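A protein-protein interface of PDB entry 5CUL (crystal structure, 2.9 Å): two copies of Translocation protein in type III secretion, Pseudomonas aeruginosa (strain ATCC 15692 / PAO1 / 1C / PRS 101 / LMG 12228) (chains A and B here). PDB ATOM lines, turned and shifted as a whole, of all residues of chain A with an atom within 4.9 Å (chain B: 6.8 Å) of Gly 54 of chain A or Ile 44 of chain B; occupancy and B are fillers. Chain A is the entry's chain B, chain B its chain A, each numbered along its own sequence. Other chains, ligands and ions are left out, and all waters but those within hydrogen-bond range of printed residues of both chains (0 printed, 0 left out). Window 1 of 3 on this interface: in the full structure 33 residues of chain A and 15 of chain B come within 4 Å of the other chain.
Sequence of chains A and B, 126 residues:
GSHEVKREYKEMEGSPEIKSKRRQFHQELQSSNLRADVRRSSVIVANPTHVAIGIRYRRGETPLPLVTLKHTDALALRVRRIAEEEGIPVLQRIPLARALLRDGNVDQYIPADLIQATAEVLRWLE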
ATOM      1  N   ALA A  52      25.642 -23.163 -12.505  1.00  0.00           N
ATOM      2  CA  ALA A  52      24.252 -23.480 -12.203  1.00  0.00           C
ATOM      3  C   ALA A  52      23.345 -22.639 -13.049  1.00  0.00           C
ATOM      4  O   ALA A  52      23.269 -21.446 -12.860  1.00  0.00           O
ATOM      5  CB  ALA A  52      23.952 -23.248 -10.745  1.00  0.00           C
ATOM      6  N   ILE A  53      22.662 -23.294 -13.981  1.00  0.00           N
ATOM      7  CA  ILE A  53      21.682 -22.670 -14.869  1.00  0.00           C
ATOM      8  C   ILE A  53      20.273 -23.176 -14.547  1.00  0.00           C
ATOM      9  O   ILE A  53      20.037 -24.371 -14.425  1.00  0.00           O
ATOM     10  CB  ILE A  53      21.977 -22.962 -16.362  1.00  0.00           C
ATOM     11  CG1 ILE A  53      23.447 -22.659 -16.721  1.00  0.00           C
ATOM     12  CG2 ILE A  53      21.028 -22.176 -17.268  1.00  0.00           C
ATOM     13  CD1 ILE A  53      23.852 -21.220 -16.503  1.00  0.00           C
ATOM     14  N   GLY A  54      19.347 -22.245 -14.406  1.00  0.00           N
ATOM     15  CA  GLY A  54      18.005 -22.568 -14.055  1.00  0.00           C
ATOM     16  C   GLY A  54      17.208 -22.605 -15.312  1.00  0.00           C
ATOM     17  O   GLY A  54      17.249 -21.671 -16.095  1.00  0.00           O
ATOM     18  N   ILE A  55      16.459 -23.686 -15.479  1.00  0.00           N
ATOM     19  CA  ILE A  55      15.594 -23.882 -16.635  1.00  0.00           C
ATOM     20  C   ILE A  55      14.140 -24.039 -16.214  1.00  0.00           C
ATOM     21  O   ILE A  55      13.823 -24.792 -15.294  1.00  0.00           O
ATOM     22  CB  ILE A  55      16.041 -25.134 -17.425  1.00  0.00           C
ATOM     23  CG1 ILE A  55      17.390 -24.892 -18.116  1.00  0.00           C
ATOM     24  CG2 ILE A  55      15.008 -25.560 -18.461  1.00  0.00           C
ATOM     25  CD1 ILE A  55      17.395 -23.725 -19.094  1.00  0.00           C
ATOM     26  N   ARG A  56      13.262 -23.330 -16.917  1.00  0.00           N
ATOM     27  CA  ARG A  56      11.813 -23.448 -16.722  1.00  0.00           C
ATOM     28  C   ARG A  56      11.114 -23.931 -17.976  1.00  0.00           C
ATOM     29  O   ARG A  56      11.304 -23.380 -19.069  1.00  0.00           O
ATOM     30  CB  ARG A  56      11.220 -22.105 -16.324  1.00  0.00           C
ATOM     31  CG  ARG A  56       9.695 -22.085 -16.282  1.00  0.00           C
ATOM     32  CD  ARG A  56       9.194 -20.717 -15.858  1.00  0.00           C
ATOM     33  NE  ARG A  56       8.620 -20.763 -14.512  1.00  0.00           N
ATOM     34  CZ  ARG A  56       7.320 -20.791 -14.267  1.00  0.00           C
ATOM     35  NH1 ARG A  56       6.475 -20.754 -15.282  1.00  0.00           N
ATOM     36  NH2 ARG A  56       6.870 -20.841 -13.013  1.00  0.00           N
ATOM     37  N   LEU A  66      12.982 -22.035 -20.818  1.00  0.00           N
ATOM     38  CA  LEU A  66      13.442 -20.678 -20.691  1.00  0.00           C
ATOM     39  C   LEU A  66      14.367 -20.592 -19.515  1.00  0.00           C
ATOM     40  O   LEU A  66      14.088 -21.155 -18.478  1.00  0.00           O
ATOM     41  CB  LEU A  66      12.214 -19.763 -20.543  1.00  0.00           C
ATOM     42  CG  LEU A  66      12.399 -18.333 -20.044  1.00  0.00           C
ATOM     43  CD1 LEU A  66      11.570 -17.353 -20.871  1.00  0.00           C
ATOM     44  CD2 LEU A  66      12.038 -18.236 -18.565  1.00  0.00           C
ATOM     45  N   VAL A  67      15.474 -19.884 -19.682  1.00  0.00           N
ATOM     46  CA  VAL A  67      16.466 -19.732 -18.606  1.00  0.00           C
ATOM     47  C   VAL A  67      15.987 -18.762 -17.546  1.00  0.00           C
ATOM     48  O   VAL A  67      15.569 -17.673 -17.867  1.00  0.00           O
ATOM     49  CB  VAL A  67      17.827 -19.238 -19.127  1.00  0.00           C
ATOM     50  CG1 VAL A  67      18.814 -19.008 -17.993  1.00  0.00           C
ATOM     51  CG2 VAL A  67      18.419 -20.232 -20.099  1.00  0.00           C
ATOM     52  N   THR A  68      16.057 -19.196 -16.290  1.00  0.00           N
ATOM     53  CA  THR A  68      15.559 -18.424 -15.142  1.00  0.00           C
ATOM     54  C   THR A  68      16.695 -17.760 -14.369  1.00  0.00           C
ATOM     55  O   THR A  68      16.485 -16.751 -13.664  1.00  0.00           O
ATOM     56  CB  THR A  68      14.720 -19.290 -14.166  1.00  0.00           C
ATOM     57  OG1 THR A  68      15.494 -20.363 -13.636  1.00  0.00           O
ATOM     58  CG2 THR A  68      13.534 -19.881 -14.879  1.00  0.00           C
ATOM     59  N   LEU A  69      17.898 -18.337 -14.499  1.00  0.00           N
ATOM     60  CA  LEU A  69      19.063 -17.867 -13.742  1.00  0.00           C
ATOM     61  C   LEU A  69      20.344 -18.463 -14.257  1.00  0.00           C
ATOM     62  O   LEU A  69      20.365 -19.554 -14.732  1.00  0.00           O
ATOM     63  CB  LEU A  69      18.904 -18.183 -12.235  1.00  0.00           C
ATOM     64  CG  LEU A  69      18.866 -19.661 -11.824  1.00  0.00           C
ATOM     65  CD1 LEU A  69      20.158 -20.078 -11.173  1.00  0.00           C
ATOM     66  CD2 LEU A  69      17.728 -19.921 -10.863  1.00  0.00           C
ATOM     67  N   VAL A  79      22.710 -21.548  -5.205  1.00  0.00           N
ATOM     68  CA  VAL A  79      21.582 -21.989  -6.006  1.00  0.00           C
ATOM     69  C   VAL A  79      21.248 -23.443  -5.780  1.00  0.00           C
ATOM     70  O   VAL A  79      20.097 -23.805  -5.679  1.00  0.00           O
ATOM     71  CB  VAL A  79      21.852 -21.766  -7.512  1.00  0.00           C
ATOM     72  CG1 VAL A  79      20.885 -22.577  -8.354  1.00  0.00           C
ATOM     73  CG2 VAL A  79      21.736 -20.279  -7.866  1.00  0.00           C
ATOM     74  N   ALA A  83      17.958 -24.972  -4.112  1.00  0.00           N
ATOM     75  CA  ALA A  83      17.212 -25.920  -4.939  1.00  0.00           C
ATOM     76  C   ALA A  83      16.833 -27.198  -4.200  1.00  0.00           C
ATOM     77  O   ALA A  83      15.753 -27.740  -4.416  1.00  0.00           O
ATOM     78  CB  ALA A  83      18.031 -26.286  -6.148  1.00  0.00           C
ATOM     79  N   ILE A  88      13.660 -28.442  -6.110  1.00  0.00           N
ATOM     80  CA  ILE A  88      14.045 -28.268  -7.512  1.00  0.00           C
ATOM     81  C   ILE A  88      15.183 -29.226  -7.846  1.00  0.00           C
ATOM     82  O   ILE A  88      16.247 -29.168  -7.221  1.00  0.00           O
ATOM     83  CB  ILE A  88      14.485 -26.837  -7.836  1.00  0.00           C
ATOM     84  CG1 ILE A  88      13.516 -25.808  -7.219  1.00  0.00           C
ATOM     85  CG2 ILE A  88      14.628 -26.679  -9.352  1.00  0.00           C
ATOM     86  CD1 ILE A  88      12.097 -25.911  -7.734  1.00  0.00           C
ATOM     87  N   PRO A  89      14.957 -30.129  -8.816  1.00  0.00           N
ATOM     88  CA  PRO A  89      15.963 -31.114  -9.185  1.00  0.00           C
ATOM     89  C   PRO A  89      17.200 -30.448  -9.759  1.00  0.00           C
ATOM     90  O   PRO A  89      17.103 -29.562 -10.581  1.00  0.00           O
ATOM     91  CB  PRO A  89      15.266 -31.990 -10.237  1.00  0.00           C
ATOM     92  CG  PRO A  89      13.815 -31.763 -10.022  1.00  0.00           C
ATOM     93  CD  PRO A  89      13.697 -30.348  -9.535  1.00  0.00           C
ATOM     94  N   VAL A  90      18.354 -30.882  -9.286  1.00  0.00           N
ATOM     95  CA  VAL A  90      19.636 -30.425  -9.803  1.00  0.00           C
ATOM     96  C   VAL A  90      20.333 -31.544 -10.575  1.00  0.00           C
ATOM     97  O   VAL A  90      20.775 -32.549 -10.007  1.00  0.00           O
ATOM     98  CB  VAL A  90      20.565 -29.950  -8.683  1.00  0.00           C
ATOM     99  CG1 VAL A  90      21.918 -29.515  -9.254  1.00  0.00           C
ATOM    100  CG2 VAL A  90      19.899 -28.836  -7.877  1.00  0.00           C
ATOM    101  N   LEU A  91      20.409 -31.363 -11.881  1.00  0.00           N
ATOM    102  CA  LEU A  91      20.973 -32.354 -12.736  1.00  0.00           C
ATOM    103  C   LEU A  91      22.338 -31.893 -13.222  1.00  0.00           C
ATOM    104  O   LEU A  91      22.508 -30.757 -13.590  1.00  0.00           O
ATOM    105  CB  LEU A  91      20.023 -32.648 -13.910  1.00  0.00           C
ATOM    106  CG  LEU A  91      19.185 -33.942 -13.806  1.00  0.00           C
ATOM    107  CD1 LEU A  91      18.252 -33.839 -12.635  1.00  0.00           C
ATOM    108  CD2 LEU A  91      18.390 -34.188 -15.084  1.00  0.00           C
ATOM    109  N   ASP B  37      14.021 -16.974  -7.833  1.00  0.00           N
ATOM    110  CA  ASP B  37      14.447 -17.421  -9.179  1.00  0.00           C
ATOM    111  C   ASP B  37      14.614 -18.918  -9.216  1.00  0.00           C
ATOM    112  O   ASP B  37      14.231 -19.550 -10.192  1.00  0.00           O
ATOM    113  CB  ASP B  37      15.756 -16.746  -9.592  1.00  0.00           C
ATOM    114  CG  ASP B  37      15.655 -15.222  -9.595  1.00  0.00           C
ATOM    115  OD1 ASP B  37      14.596 -14.732 -10.065  1.00  0.00           O
ATOM    116  OD2 ASP B  37      16.609 -14.536  -9.120  1.00  0.00           O
ATOM    117  N   VAL B  38      15.166 -19.464  -8.131  1.00  0.00           N
ATOM    118  CA  VAL B  38      15.338 -20.910  -7.971  1.00  0.00           C
ATOM    119  C   VAL B  38      13.990 -21.611  -7.962  1.00  0.00           C
ATOM    120  O   VAL B  38      13.831 -22.688  -8.510  1.00  0.00           O
ATOM    121  CB  VAL B  38      16.124 -21.272  -6.672  1.00  0.00           C
ATOM    122  CG1 VAL B  38      16.320 -22.779  -6.550  1.00  0.00           C
ATOM    123  CG2 VAL B  38      17.500 -20.603  -6.644  1.00  0.00           C
ATOM    124  N   SER B  41      12.198 -22.184 -11.264  1.00  0.00           N
ATOM    125  CA  SER B  41      12.848 -23.185 -12.104  1.00  0.00           C
ATOM    126  C   SER B  41      12.203 -24.563 -12.018  1.00  0.00           C
ATOM    127  O   SER B  41      11.701 -24.968 -10.978  1.00  0.00           O
ATOM    128  CB  SER B  41      14.336 -23.297 -11.746  1.00  0.00           C
ATOM    129  OG  SER B  41      14.976 -22.029 -11.731  1.00  0.00           O
ATOM    130  N   SER B  42      12.224 -25.268 -13.143  1.00  0.00           N
ATOM    131  CA  SER B  42      11.748 -26.641 -13.215  1.00  0.00           C
ATOM    132  C   SER B  42      12.915 -27.589 -12.910  1.00  0.00           C
ATOM    133  O   SER B  42      12.731 -28.701 -12.383  1.00  0.00           O
ATOM    134  CB  SER B  42      11.138 -26.934 -14.615  1.00  0.00           C
ATOM    135  OG  SER B  42      10.149 -25.973 -15.000  1.00  0.00           O
ATOM    136  N   VAL B  43      14.115 -27.134 -13.250  1.00  0.00           N
ATOM    137  CA  VAL B  43      15.315 -27.937 -13.099  1.00  0.00           C
ATOM    138  C   VAL B  43      16.541 -27.050 -13.138  1.00  0.00           C
ATOM    139  O   VAL B  43      16.557 -26.041 -13.819  1.00  0.00           O
ATOM    140  CB  VAL B  43      15.421 -28.996 -14.224  1.00  0.00           C
ATOM    141  CG1 VAL B  43      15.403 -28.343 -15.618  1.00  0.00           C
ATOM    142  CG2 VAL B  43      16.671 -29.866 -14.044  1.00  0.00           C
ATOM    143  N   ILE B  44      17.561 -27.429 -12.389  1.00  0.00           N
ATOM    144  CA  ILE B  44      18.826 -26.699 -12.397  1.00  0.00           C
ATOM    145  C   ILE B  44      19.821 -27.570 -13.133  1.00  0.00           C
ATOM    146  O   ILE B  44      20.006 -28.735 -12.820  1.00  0.00           O
ATOM    147  CB  ILE B  44      19.355 -26.382 -10.965  1.00  0.00           C
ATOM    148  CG1 ILE B  44      18.325 -25.581 -10.132  1.00  0.00           C
ATOM    149  CG2 ILE B  44      20.680 -25.642 -11.030  1.00  0.00           C
ATOM    150  CD1 ILE B  44      18.163 -24.145 -10.535  1.00  0.00           C
ATOM    151  N   VAL B  45      20.463 -27.001 -14.123  1.00  0.00           N
ATOM    152  CA  VAL B  45      21.504 -27.704 -14.806  1.00  0.00           C
ATOM    153  C   VAL B  45      22.833 -27.270 -14.217  1.00  0.00           C
ATOM    154  O   VAL B  45      23.171 -26.122 -14.235  1.00  0.00           O
ATOM    155  CB  VAL B  45      21.494 -27.397 -16.307  1.00  0.00           C
ATOM    156  CG1 VAL B  45      22.527 -28.248 -17.032  1.00  0.00           C
ATOM    157  CG2 VAL B  45      20.125 -27.666 -16.894  1.00  0.00           C
ATOM    158  N   ALA B  46      23.598 -28.226 -13.734  1.00  0.00           N
ATOM    159  CA  ALA B  46      24.871 -27.950 -13.158  1.00  0.00           C
ATOM    160  C   ALA B  46      25.971 -28.687 -13.920  1.00  0.00           C
ATOM    161  O   ALA B  46      25.700 -29.544 -14.729  1.00  0.00           O
ATOM    162  CB  ALA B  46      24.846 -28.362 -11.674  1.00  0.00           C
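The side-chain hydroxyl of Thr 68 of chain A is in hydrogen-bond range of the side-chain hydroxyl of Ser 41 of chain B (2.6 Å). The backbone NH (N) of Ser 42 of chain B is in hydrogen-bond range of the backbone carbonyl oxygen (O) of Ile 55 of chain A, 2.7 Å away. The backbone carbonyl oxygen (O) of Val 43 of chain B lies within hydrogen-bond range of the backbone NH (N) of Ile 55 of chain A, 2.9 Å away. The backbone carbonyl oxygen of Pro 89 of chain A lies within hydrogen-bond range of the backbone NH of Ile 44 of chain B, 2.8 Å away. O of Ile 44 of chain B sits at hydrogen-bond distance from N of Leu 91 of chain A (2.8 Å). The backbone carbonyl oxygen (O) of Ile 53 of chain A is in hydrogen-bond range of the backbone NH (N) of Val 45 of chain B (2.7 Å). N of Ala 46 of chain B sits at hydrogen-bond distance from O of Leu 91 of chain A, 2.8 Å away.
O of Asp 37 of chain B lies within hydrogen-bond range of OG of Ser 41 of chain B (3.0 Å). O of Val 38 of chain B sits close to OG of Ser 41 of chain B (3.5 Å). The backbone carbonyl oxygen (O) of Gly 54 of chain A is in hydrogen-bond range of the backbone NH (N) of Thr 68 of chain A, at 2.8 Å. The backbone carbonyl oxygen (O) of Leu 69 of chain A sits at hydrogen-bond distance from the backbone NH (N) of Gly 54 of chain A, 2.9 Å away. The backbone NH of Leu 66 of chain A is in hydrogen-bond range of the backbone carbonyl oxygen of Arg 56 of chain A, at 2.8 Å. The backbone carbonyl oxygen of Ala 83 of chain A is in hydrogen-bond range of the backbone NH of Ile 88 of chain A.
Ala 52 of chain A touches Val 45 of chain B. Ile 44 of chain B touches Ile 53 of chain A (CA to O, 3.3 Å). O of Ile 55 of chain A touches C of Ser 41 of chain B, at 3.7 Å. Asp 37 of chain B touches Thr 68 of chain A. Asp 37 of chain B touches Leu 69 of chain A (O to CD2, 3.6 Å). CG1 of Val 79 of chain A touches CD1 of Ile 44 of chain B, 3.8 Å away. CG1 of Val 38 of chain B touches CA of Ala 83 of chain A, 3.6 Å away. Ile 88 of chain A touches Val 43 of chain B (CG2 to N, 3.96 Å). Ile 44 of chain B touches Val 90 of chain A. Val 90 of chain A touches Ala 46 of chain B (CG1 to CB, 3.97 Å).
Gly 54 of chain A touches just these residues of chain B: Ser 41, Val 43 and Ile 44. Of chain A, only Ile 53, Gly 54, Val 79, Ile 88, Pro 89, Val 90 and Leu 91 come within 4 Å of Ile 44 of chain B. Of the printed residues of chain B, Leu 91 of chain A touches Ile 44, Val 45 and Ala 46. Of the printed residues of chain B, Ala 83 of chain A touches Val 38. The nearest residue of chain B that does not touch Gly 54 of chain A is Val 45 of chain B (4.9 Å). The nearest printed residue of chain A that does not touch Ile 44 of chain B is Ala 83 of chain A (4.1 Å). The nearest printed residue of chain A that does not touch Ser 42 of chain B is Ile 88 of chain A (4.1 Å).
Of the 15 printed residues of chain A, 13 touch a printed residue of chain B. Hydrophobic or aromatic side chains of chain A that line the printed part of chain B: Ile 53, Ile 55, Leu 69, Val 79, Ala 83, Ile 88, Pro 89 and Val 90. Among the printed residues, 30 pairs touch across the chains. Among the printed residues, no Asp or Glu carboxylate lies within 4 Å of a Lys or Arg side-chain nitrogen of the other chain.
No position is printed for both chains.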
